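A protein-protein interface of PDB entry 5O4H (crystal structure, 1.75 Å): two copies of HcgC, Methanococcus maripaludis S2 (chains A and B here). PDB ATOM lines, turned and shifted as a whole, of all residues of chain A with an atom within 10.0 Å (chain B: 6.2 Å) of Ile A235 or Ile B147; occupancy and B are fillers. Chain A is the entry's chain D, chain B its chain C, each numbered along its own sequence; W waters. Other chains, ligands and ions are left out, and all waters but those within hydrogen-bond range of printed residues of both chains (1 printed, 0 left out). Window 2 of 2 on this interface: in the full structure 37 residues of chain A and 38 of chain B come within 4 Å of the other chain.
Among the printed residues, merely in contact across the chains: Leu A199 with Ile B144, Ser A8 with Gly B116, Thr A6 with Gly B116, Val A198 with Ile B144, Asp A196 with Lys B142, Ser A8 with Ile B147, Thr A6 with Ile B115, Val A9 with Ile B115, Leu A199 with Ile B115, Ile A235 with Ile B147 and Leu A195 with Asp B141.
Water W1 bridges O of Gly B116 and OG of Ser A8.
The side-chain carboxylate of Asp B141 lies within hydrogen-bond range of the backbone NH of Ser A197. The backbone NH (N) of Gly B143 lies within hydrogen-bond range of the side-chain carboxylate (OD1) of Asp A196, at 3.1 Å. The side-chain carboxylate (OD1) of Asp A196 lies close to the side-chain carboxylate (OD1) of Asp B141, at 3.1 Å.
Printed residues of chain A that touch a printed residue of chain B: Thr A6, Ser A8, Val A9, Leu A195, Asp A196, Ser A197, Val A198, Leu A199 and Ile A235. Hydrophobic or aromatic side chains of chain B within 4 Å of the printed part of chain A: Ile B115, Ile B144 and Ile B147.
Ile A235 touches just one residue of chain B: Ile B147 (3.9 Å). Of chain A, only Ser A8 (3.7 Å) and Ile A235 (3.9 Å) come within 4 Å of Ile B147. Of the printed residues of chain B, Val A9 touches Ile B115. Of the printed residues of chain A, Lys B142 touches Asp A196 (3.7 Å). Of the printed residues of chain A, Gly B116 touches Thr A6 (3.5 Å) and Ser A8 (3.4 Å). Of the printed residues of chain A, Asp B141 touches Leu A195, Asp A196 and Ser A197. Ile A192 touches none of the printed residues of chain B. Asn B149 touches none of the printed residues of chain A. The nearest residue of chain B that does not touch Ile A235 is Ile B115 (4.1 Å). The nearest residue of chain A that does not touch Ile B147 is Val A9 (5.6 Å). The nearest printed residue of chain B that does not touch Asp A196 is Ile B144 (5.0 Å).
No position is printed for both chains.
The side-chain carboxylate (OD1) of Asp B141 lies within hydrogen-bond range of the backbone NH (N) of Gly B143, 3.0 Å away. The backbone NH (N) of Ile B144 lies within hydrogen-bond range of the side-chain carboxylate (OD1) of Asp B141 (2.8 Å). OG1 of Thr A6 sits close to N of Ser A8, 3.3 Å away. The backbone NH (N) of Ile A235 is in hydrogen-bond range of the backbone carbonyl oxygen (O) of Ser A197 (2.9 Å). The side-chain hydroxyl (OG) of Ser A197 lies within hydrogen-bond range of the backbone NH (N) of Asp A236, 3.0 Å away. N of Leu A199 lies within hydrogen-bond range of O of Ser A233 (2.8 Å).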
ATOM      1  N   THR A   6      -2.977   5.409  28.067  1.00  0.00           N
ATOM      2  CA  THR A   6      -1.679   4.826  28.431  1.00  0.00           C
ATOM      3  C   THR A   6      -1.179   3.925  27.298  1.00  0.00           C
ATOM      4  O   THR A   6      -1.912   3.679  26.341  1.00  0.00           O
ATOM      5  CB  THR A   6      -1.803   3.987  29.725  1.00  0.00           C
ATOM      6  OG1 THR A   6      -2.529   2.780  29.450  1.00  0.00           O
ATOM      7  CG2 THR A   6      -2.432   4.775  30.884  1.00  0.00           C
ATOM      8  N   GLU A   7       0.056   3.418  27.424  1.00  0.00           N
ATOM      9  CA  GLU A   7       0.651   2.530  26.416  1.00  0.00           C
ATOM     10  C   GLU A   7       0.144   1.065  26.524  1.00  0.00           C
ATOM     11  O   GLU A   7       0.555   0.220  25.730  1.00  0.00           O
ATOM     12  CB  GLU A   7       2.186   2.606  26.468  1.00  0.00           C
ATOM     13  CG  GLU A   7       2.699   4.005  26.164  1.00  0.00           C
ATOM     14  CD  GLU A   7       4.204   4.129  26.035  1.00  0.00           C
ATOM     15  OE1 GLU A   7       4.660   4.899  25.160  1.00  0.00           O
ATOM     16  OE2 GLU A   7       4.929   3.475  26.819  1.00  0.00           O
ATOM     17  N   SER A   8      -0.743   0.765  27.497  1.00  0.00           N
ATOM     18  CA  SER A   8      -1.299  -0.579  27.679  1.00  0.00           C
ATOM     19  C   SER A   8      -2.500  -0.764  26.735  1.00  0.00           C
ATOM     20  O   SER A   8      -2.944  -1.885  26.499  1.00  0.00           O
ATOM     21  CB  SER A   8      -1.802  -0.736  29.115  1.00  0.00           C
ATOM     22  OG  SER A   8      -0.739  -0.631  30.052  1.00  0.00           O
ATOM     23  N   VAL A   9      -3.035   0.341  26.235  1.00  0.00           N
ATOM     24  CA  VAL A   9      -4.180   0.355  25.366  1.00  0.00           C
ATOM     25  C   VAL A   9      -3.816   0.990  24.040  1.00  0.00           C
ATOM     26  O   VAL A   9      -3.183   2.030  24.005  1.00  0.00           O
ATOM     27  CB  VAL A   9      -5.327   1.135  26.079  1.00  0.00           C
ATOM     28  CG1 VAL A   9      -6.584   1.176  25.228  1.00  0.00           C
ATOM     29  CG2 VAL A   9      -5.636   0.518  27.445  1.00  0.00           C
ATOM     30  N   LYS A  10      -4.247   0.366  22.952  1.00  0.00           N
ATOM     31  CA  LYS A  10      -4.001   0.833  21.603  1.00  0.00           C
ATOM     32  C   LYS A  10      -5.214   1.543  21.054  1.00  0.00           C
ATOM     33  O   LYS A  10      -6.326   1.138  21.350  1.00  0.00           O
ATOM     34  CB  LYS A  10      -3.712  -0.367  20.687  1.00  0.00           C
ATOM     35  CG  LYS A  10      -2.571  -1.242  21.139  1.00  0.00           C
ATOM     36  CD  LYS A  10      -2.442  -2.463  20.250  1.00  0.00           C
ATOM     37  CE  LYS A  10      -1.338  -3.404  20.701  1.00  0.00           C
ATOM     38  NZ  LYS A  10      -0.004  -2.762  20.675  1.00  0.00           N
ATOM     39  N   THR A  11      -5.009   2.590  20.262  1.00  0.00           N
ATOM     40  CA  THR A  11      -6.073   3.338  19.612  1.00  0.00           C
ATOM     41  C   THR A  11      -5.830   3.111  18.149  1.00  0.00           C
ATOM     42  O   THR A  11      -4.730   3.376  17.687  1.00  0.00           O
ATOM     43  CB  THR A  11      -6.033   4.829  19.893  1.00  0.00           C
ATOM     44  OG1 THR A  11      -6.228   5.012  21.281  1.00  0.00           O
ATOM     45  CG2 THR A  11      -7.111   5.588  19.104  1.00  0.00           C
ATOM     46  N   THR A  12      -6.831   2.632  17.435  1.00  0.00           N
ATOM     47  CA  THR A  12      -6.731   2.352  16.009  1.00  0.00           C
ATOM     48  C   THR A  12      -7.852   3.057  15.275  1.00  0.00           C
ATOM     49  O   THR A  12      -9.012   2.896  15.617  1.00  0.00           O
ATOM     50  CB  THR A  12      -6.804   0.815  15.768  1.00  0.00           C
ATOM     51  OG1 THR A  12      -5.832   0.169  16.589  1.00  0.00           O
ATOM     52  CG2 THR A  12      -6.547   0.424  14.308  1.00  0.00           C
ATOM     53  N   ILE A 192     -17.369  -5.122  15.648  1.00  0.00           N
ATOM     54  CA  ILE A 192     -16.011  -4.827  16.103  1.00  0.00           C
ATOM     55  C   ILE A 192     -15.965  -4.849  17.625  1.00  0.00           C
ATOM     56  O   ILE A 192     -14.989  -5.335  18.204  1.00  0.00           O
ATOM     57  CB  ILE A 192     -15.531  -3.468  15.540  1.00  0.00           C
ATOM     58  CG1 ILE A 192     -15.250  -3.586  14.037  1.00  0.00           C
ATOM     59  CG2 ILE A 192     -14.275  -2.964  16.266  1.00  0.00           C
ATOM     60  CD1 ILE A 192     -15.337  -2.268  13.290  1.00  0.00           C
ATOM     61  N   LEU A 195     -15.075  -8.115  19.293  1.00  0.00           N
ATOM     62  CA  LEU A 195     -13.789  -8.721  19.049  1.00  0.00           C
ATOM     63  C   LEU A 195     -13.090  -8.790  20.397  1.00  0.00           C
ATOM     64  O   LEU A 195     -13.229  -7.874  21.217  1.00  0.00           O
ATOM     65  CB  LEU A 195     -12.918  -7.869  18.130  1.00  0.00           C
ATOM     66  CG  LEU A 195     -13.297  -7.780  16.655  1.00  0.00           C
ATOM     67  CD1 LEU A 195     -12.501  -6.674  15.962  1.00  0.00           C
ATOM     68  CD2 LEU A 195     -13.035  -9.063  15.953  1.00  0.00           C
ATOM     69  N   ASP A 196     -12.324  -9.857  20.642  1.00  0.00           N
ATOM     70  CA  ASP A 196     -11.612  -9.963  21.897  1.00  0.00           C
ATOM     71  C   ASP A 196     -10.639  -8.803  22.044  1.00  0.00           C
ATOM     72  O   ASP A 196     -10.029  -8.375  21.068  1.00  0.00           O
ATOM     73  CB  ASP A 196     -10.801 -11.274  21.956  1.00  0.00           C
ATOM     74  CG  ASP A 196      -9.920 -11.379  23.193  1.00  0.00           C
ATOM     75  OD1 ASP A 196     -10.430 -11.142  24.318  1.00  0.00           O
ATOM     76  OD2 ASP A 196      -8.697 -11.619  23.036  1.00  0.00           O
ATOM     77  N   SER A 197     -10.499  -8.292  23.277  1.00  0.00           N
ATOM     78  CA  SER A 197      -9.607  -7.214  23.679  1.00  0.00           C
ATOM     79  C   SER A 197     -10.102  -5.823  23.369  1.00  0.00           C
ATOM     80  O   SER A 197      -9.462  -4.884  23.818  1.00  0.00           O
ATOM     81  CB  SER A 197      -8.200  -7.425  23.109  1.00  0.00           C
ATOM     82  OG  SER A 197      -8.029  -6.734  21.881  1.00  0.00           O
ATOM     83  N   VAL A 198     -11.228  -5.654  22.646  1.00  0.00           N
ATOM     84  CA  VAL A 198     -11.725  -4.320  22.359  1.00  0.00           C
ATOM     85  C   VAL A 198     -12.397  -3.722  23.613  1.00  0.00           C
ATOM     86  O   VAL A 198     -13.239  -4.395  24.228  1.00  0.00           O
ATOM     87  CB  VAL A 198     -12.691  -4.324  21.145  1.00  0.00           C
ATOM     88  CG1 VAL A 198     -13.411  -2.980  21.000  1.00  0.00           C
ATOM     89  CG2 VAL A 198     -11.908  -4.644  19.867  1.00  0.00           C
ATOM     90  N   LEU A 199     -12.032  -2.478  23.966  1.00  0.00           N
ATOM     91  CA  LEU A 199     -12.592  -1.745  25.115  1.00  0.00           C
ATOM     92  C   LEU A 199     -13.825  -1.000  24.664  1.00  0.00           C
ATOM     93  O   LEU A 199     -14.863  -1.013  25.332  1.00  0.00           O
ATOM     94  CB  LEU A 199     -11.609  -0.689  25.684  1.00  0.00           C
ATOM     95  CG  LEU A 199     -10.255  -1.113  26.273  1.00  0.00           C
ATOM     96  CD1 LEU A 199      -9.735  -0.048  27.235  1.00  0.00           C
ATOM     97  CD2 LEU A 199     -10.340  -2.410  27.019  1.00  0.00           C
ATOM     98  N   TYR A 200     -13.716  -0.301  23.532  1.00  0.00           N
ATOM     99  CA  TYR A 200     -14.794   0.445  22.976  1.00  0.00           C
ATOM    100  C   TYR A 200     -14.541   0.740  21.521  1.00  0.00           C
ATOM    101  O   TYR A 200     -13.400   0.671  21.048  1.00  0.00           O
ATOM    102  CB  TYR A 200     -15.174   1.703  23.779  1.00  0.00           C
ATOM    103  CG  TYR A 200     -14.167   2.821  23.737  1.00  0.00           C
ATOM    104  CD1 TYR A 200     -14.115   3.685  22.661  1.00  0.00           C
ATOM    105  CD2 TYR A 200     -13.326   3.065  24.807  1.00  0.00           C
ATOM    106  CE1 TYR A 200     -13.214   4.740  22.627  1.00  0.00           C
ATOM    107  CE2 TYR A 200     -12.424   4.114  24.791  1.00  0.00           C
ATOM    108  CZ  TYR A 200     -12.376   4.959  23.698  1.00  0.00           C
ATOM    109  OH  TYR A 200     -11.502   6.006  23.656  1.00  0.00           O
ATOM    110  N   VAL A 232     -11.180   2.578  17.300  1.00  0.00           N
ATOM    111  CA  VAL A 232     -11.263   1.470  18.237  1.00  0.00           C
ATOM    112  C   VAL A 232     -10.194   1.567  19.299  1.00  0.00           C
ATOM    113  O   VAL A 232      -9.050   1.896  19.007  1.00  0.00           O
ATOM    114  CB  VAL A 232     -11.105   0.106  17.504  1.00  0.00           C
ATOM    115  CG1 VAL A 232     -11.471  -1.061  18.422  1.00  0.00           C
ATOM    116  CG2 VAL A 232     -11.950   0.064  16.237  1.00  0.00           C
ATOM    117  N   SER A 233     -10.572   1.237  20.534  1.00  0.00           N
ATOM    118  CA  SER A 233      -9.675   1.209  21.683  1.00  0.00           C
ATOM    119  C   SER A 233      -9.566  -0.254  22.026  1.00  0.00           C
ATOM    120  O   SER A 233     -10.595  -0.898  22.232  1.00  0.00           O
ATOM    121  CB  SER A 233     -10.230   2.049  22.834  1.00  0.00           C
ATOM    122  OG  SER A 233      -9.339   1.999  23.922  1.00  0.00           O
ATOM    123  N   SER A 234      -8.365  -0.827  22.070  1.00  0.00           N
ATOM    124  CA  SER A 234      -8.199  -2.251  22.363  1.00  0.00           C
ATOM    125  C   SER A 234      -6.870  -2.584  22.988  1.00  0.00           C
ATOM    126  O   SER A 234      -5.945  -1.776  22.964  1.00  0.00           O
ATOM    127  CB  SER A 234      -8.361  -3.041  21.060  1.00  0.00           C
ATOM    128  OG  SER A 234      -7.297  -2.745  20.165  1.00  0.00           O
ATOM    129  N   ILE A 235      -6.751  -3.787  23.560  1.00  0.00           N
ATOM    130  CA  ILE A 235      -5.496  -4.222  24.171  1.00  0.00           C
ATOM    131  C   ILE A 235      -4.634  -4.864  23.074  1.00  0.00           C
ATOM    132  O   ILE A 235      -3.420  -4.707  23.098  1.00  0.00           O
ATOM    133  CB  ILE A 235      -5.685  -5.227  25.339  1.00  0.00           C
ATOM    134  CG1 ILE A 235      -6.647  -4.693  26.411  1.00  0.00           C
ATOM    135  CG2 ILE A 235      -4.336  -5.612  25.954  1.00  0.00           C
ATOM    136  CD1 ILE A 235      -6.290  -3.322  26.965  1.00  0.00           C
ATOM    137  N   ASP A 236      -5.250  -5.597  22.134  1.00  0.00           N
ATOM    138  CA  ASP A 236      -4.522  -6.272  21.050  1.00  0.00           C
ATOM    139  C   ASP A 236      -4.671  -5.555  19.722  1.00  0.00           C
ATOM    140  O   ASP A 236      -5.531  -4.703  19.559  1.00  0.00           O
ATOM    141  CB  ASP A 236      -5.048  -7.715  20.884  1.00  0.00           C
ATOM    142  CG  ASP A 236      -4.932  -8.604  22.119  1.00  0.00           C
ATOM    143  OD1 ASP A 236      -4.236  -8.212  23.069  1.00  0.00           O
ATOM    144  OD2 ASP A 236      -5.561  -9.681  22.131  1.00  0.00           O
ATOM    145  N   HIS A 237      -3.823  -5.935  18.748  1.00  0.00           N
ATOM    146  CA  HIS A 237      -3.877  -5.344  17.410  1.00  0.00           C
ATOM    147  C   HIS A 237      -5.159  -5.825  16.775  1.00  0.00           C
ATOM    148  O   HIS A 237      -5.471  -7.011  16.861  1.00  0.00           O
ATOM    149  CB  HIS A 237      -2.683  -5.774  16.547  1.00  0.00           C
ATOM    150  CG  HIS A 237      -1.389  -5.251  17.059  1.00  0.00           C
ATOM    151  ND1 HIS A 237      -1.091  -3.898  17.012  1.00  0.00           N
ATOM    152  CD2 HIS A 237      -0.350  -5.913  17.620  1.00  0.00           C
ATOM    153  CE1 HIS A 237       0.116  -3.784  17.547  1.00  0.00           C
ATOM    154  NE2 HIS A 237       0.597  -4.973  17.925  1.00  0.00           N
ATOM    155  N   VAL A 238      -5.907  -4.918  16.161  1.00  0.00           N
ATOM    156  CA  VAL A 238      -7.183  -5.245  15.510  1.00  0.00           C
ATOM    157  C   VAL A 238      -7.282  -4.645  14.109  1.00  0.00           C
ATOM    158  O   VAL A 238      -8.347  -4.698  13.548  1.00  0.00           O
ATOM    159  CB  VAL A 238      -8.392  -4.774  16.370  1.00  0.00           C
ATOM    160  CG1 VAL A 238      -8.482  -5.544  17.674  1.00  0.00           C
ATOM    161  CG2 VAL A 238      -8.369  -3.275  16.613  1.00  0.00           C
ATOM    162  N   GLU A 239      -6.190  -4.097  13.540  1.00  0.00           N
ATOM    163  CA  GLU A 239      -6.228  -3.478  12.215  1.00  0.00           C
ATOM    164  C   GLU A 239      -6.815  -4.381  11.126  1.00  0.00           C
ATOM    165  O   GLU A 239      -7.671  -3.942  10.391  1.00  0.00           O
ATOM    166  CB  GLU A 239      -4.830  -2.998  11.801  1.00  0.00           C
ATOM    167  CG  GLU A 239      -4.316  -1.864  12.668  1.00  0.00           C
ATOM    168  CD  GLU A 239      -2.824  -1.819  12.927  1.00  0.00           C
ATOM    169  OE1 GLU A 239      -2.119  -2.842  12.784  1.00  0.00           O
ATOM    170  OE2 GLU A 239      -2.336  -0.676  13.058  1.00  0.00           O
ATOM    171  N   ILE B 115      -7.222   0.464  33.570  1.00  0.00           N
ATOM    172  CA  ILE B 115      -6.219  -0.263  32.776  1.00  0.00           C
ATOM    173  C   ILE B 115      -4.962   0.525  32.539  1.00  0.00           C
ATOM    174  O   ILE B 115      -5.018   1.638  32.054  1.00  0.00           O
ATOM    175  CB  ILE B 115      -6.788  -0.821  31.451  1.00  0.00           C
ATOM    176  CG1 ILE B 115      -7.968  -1.794  31.689  1.00  0.00           C
ATOM    177  CG2 ILE B 115      -5.679  -1.541  30.656  1.00  0.00           C
ATOM    178  CD1 ILE B 115      -8.919  -1.840  30.540  1.00  0.00           C
ATOM    179  N   GLY B 116      -3.830  -0.077  32.887  1.00  0.00           N
ATOM    180  CA  GLY B 116      -2.513   0.540  32.727  1.00  0.00           C
ATOM    181  C   GLY B 116      -2.259   1.726  33.625  1.00  0.00           C
ATOM    182  O   GLY B 116      -1.361   2.513  33.352  1.00  0.00           O
ATOM    183  N   ASP B 141     -14.100 -10.414  29.137  1.00  0.00           N
ATOM    184  CA  ASP B 141     -13.272 -10.344  27.933  1.00  0.00           C
ATOM    185  C   ASP B 141     -11.906 -10.912  28.369  1.00  0.00           C
ATOM    186  O   ASP B 141     -11.270 -10.392  29.276  1.00  0.00           O
ATOM    187  CB  ASP B 141     -13.218  -8.932  27.356  1.00  0.00           C
ATOM    188  CG  ASP B 141     -12.280  -8.800  26.155  1.00  0.00           C
ATOM    189  OD1 ASP B 141     -11.053  -8.851  26.352  1.00  0.00           O
ATOM    190  OD2 ASP B 141     -12.780  -8.587  25.030  1.00  0.00           O
ATOM    191  N   LYS B 142     -11.459 -11.999  27.733  1.00  0.00           N
ATOM    192  CA  LYS B 142     -10.179 -12.645  28.039  1.00  0.00           C
ATOM    193  C   LYS B 142      -8.991 -11.693  28.000  1.00  0.00           C
ATOM    194  O   LYS B 142      -8.191 -11.715  28.912  1.00  0.00           O
ATOM    195  CB  LYS B 142      -9.901 -13.793  27.066  1.00  0.00           C
ATOM    196  CG  LYS B 142     -10.699 -15.013  27.345  1.00  0.00           C
ATOM    197  CD  LYS B 142     -10.187 -16.131  26.448  1.00  0.00           C
ATOM    198  CE  LYS B 142     -10.979 -17.395  26.506  1.00  0.00           C
ATOM    199  NZ  LYS B 142     -12.284 -17.322  25.776  1.00  0.00           N
ATOM    200  N   GLY B 143      -8.902 -10.887  26.961  1.00  0.00           N
ATOM    201  CA  GLY B 143      -7.815  -9.927  26.802  1.00  0.00           C
ATOM    202  C   GLY B 143      -7.802  -8.886  27.907  1.00  0.00           C
ATOM    203  O   GLY B 143      -6.751  -8.623  28.500  1.00  0.00           O
ATOM    204  N   ILE B 144      -8.978  -8.281  28.208  1.00  0.00           N
ATOM    205  CA  ILE B 144      -9.105  -7.250  29.244  1.00  0.00           C
ATOM    206  C   ILE B 144      -8.857  -7.874  30.614  1.00  0.00           C
ATOM    207  O   ILE B 144      -8.183  -7.277  31.441  1.00  0.00           O
ATOM    208  CB  ILE B 144     -10.475  -6.506  29.169  1.00  0.00           C
ATOM    209  CG1 ILE B 144     -10.592  -5.706  27.866  1.00  0.00           C
ATOM    210  CG2 ILE B 144     -10.690  -5.563  30.356  1.00  0.00           C
ATOM    211  CD1 ILE B 144     -12.025  -5.268  27.447  1.00  0.00           C
ATOM    212  N   SER B 145      -9.399  -9.069  30.872  1.00  0.00           N
ATOM    213  CA  SER B 145      -9.207  -9.721  32.167  1.00  0.00           C
ATOM    214  C   SER B 145      -7.724 -10.016  32.464  1.00  0.00           C
ATOM    215  O   SER B 145      -7.302  -9.914  33.612  1.00  0.00           O
ATOM    216  CB  SER B 145      -9.996 -11.011  32.218  1.00  0.00           C
ATOM    217  OG  SER B 145     -10.032 -11.549  33.517  1.00  0.00           O
ATOM    218  N   LYS B 146      -6.946 -10.356  31.434  1.00  0.00           N
ATOM    219  CA  LYS B 146      -5.525 -10.656  31.607  1.00  0.00           C
ATOM    220  C   LYS B 146      -4.713  -9.395  32.002  1.00  0.00           C
ATOM    221  O   LYS B 146      -3.909  -9.472  32.919  1.00  0.00           O
ATOM    222  CB  LYS B 146      -4.994 -11.268  30.312  1.00  0.00           C
ATOM    223  CG  LYS B 146      -3.501 -11.564  30.276  1.00  0.00           C
ATOM    224  CD  LYS B 146      -3.068 -12.470  31.399  1.00  0.00           C
ATOM    225  CE  LYS B 146      -1.633 -12.888  31.258  1.00  0.00           C
ATOM    226  NZ  LYS B 146      -1.209 -13.687  32.418  1.00  0.00           N
ATOM    227  N   ILE B 147      -4.918  -8.253  31.326  1.00  0.00           N
ATOM    228  CA  ILE B 147      -4.180  -7.018  31.642  1.00  0.00           C
ATOM    229  C   ILE B 147      -4.641  -6.347  32.938  1.00  0.00           C
ATOM    230  O   ILE B 147      -3.907  -5.537  33.526  1.00  0.00           O
ATOM    231  CB  ILE B 147      -4.228  -6.031  30.441  1.00  0.00           C
ATOM    232  CG1 ILE B 147      -3.090  -4.991  30.551  1.00  0.00           C
ATOM    233  CG2 ILE B 147      -5.587  -5.331  30.293  1.00  0.00           C
ATOM    234  CD1 ILE B 147      -2.720  -4.385  29.263  1.00  0.00           C
ATOM    235  N   ASP B 148      -5.859  -6.648  33.383  1.00  0.00           N
ATOM    236  CA  ASP B 148      -6.405  -6.085  34.589  1.00  0.00           C
ATOM    237  C   ASP B 148      -5.655  -6.577  35.839  1.00  0.00           C
ATOM    238  O   ASP B 148      -5.375  -7.758  35.944  1.00  0.00           O
ATOM    239  CB  ASP B 148      -7.882  -6.458  34.716  1.00  0.00           C
ATOM    240  CG  ASP B 148      -8.454  -6.022  36.037  1.00  0.00           C
ATOM    241  OD1 ASP B 148      -8.457  -4.812  36.299  1.00  0.00           O
ATOM    242  OD2 ASP B 148      -8.790  -6.910  36.858  1.00  0.00           O
ATOM    243  N   ASN B 149      -5.339  -5.692  36.779  1.00  0.00           N
ATOM    244  CA  ASN B 149      -4.652  -6.084  38.020  1.00  0.00           C
ATOM    245  C   ASN B 149      -5.340  -5.445  39.238  1.00  0.00           C
ATOM    246  O   ASN B 149      -4.693  -5.186  40.253  1.00  0.00           O
ATOM    247  CB  ASN B 149      -3.165  -5.755  37.965  1.00  0.00           C
ATOM    248  CG  ASN B 149      -2.856  -4.284  37.921  1.00  0.00           C
ATOM    249  OD1 ASN B 149      -3.717  -3.449  37.687  1.00  0.00           O
ATOM    250  ND2 ASN B 149      -1.616  -3.921  38.150  1.00  0.00           N
ATOM    251  N   ARG B 153      -4.013  -4.328  43.256  1.00  0.00           N
ATOM    252  CA  ARG B 153      -4.029  -2.954  43.772  1.00  0.00           C
ATOM    253  C   ARG B 153      -4.715  -2.857  45.115  1.00  0.00           C
ATOM    254  O   ARG B 153      -4.463  -1.900  45.841  1.00  0.00           O
ATOM    255  CB  ARG B 153      -4.726  -2.004  42.803  1.00  0.00           C
ATOM    256  CG  ARG B 153      -3.985  -1.842  41.517  1.00  0.00           C
ATOM    257  CD  ARG B 153      -4.675  -0.842  40.599  1.00  0.00           C
ATOM    258  NE  ARG B 153      -4.353  -1.125  39.207  1.00  0.00           N
ATOM    259  CZ  ARG B 153      -4.622  -0.342  38.171  1.00  0.00           C
ATOM    260  NH1 ARG B 153      -5.230   0.820  38.348  1.00  0.00           N
ATOM    261  NH2 ARG B 153      -4.278  -0.713  36.949  1.00  0.00           N
HETATM  262  O   HOH W   1       0.466   1.656  31.531  1.00  0.00           O
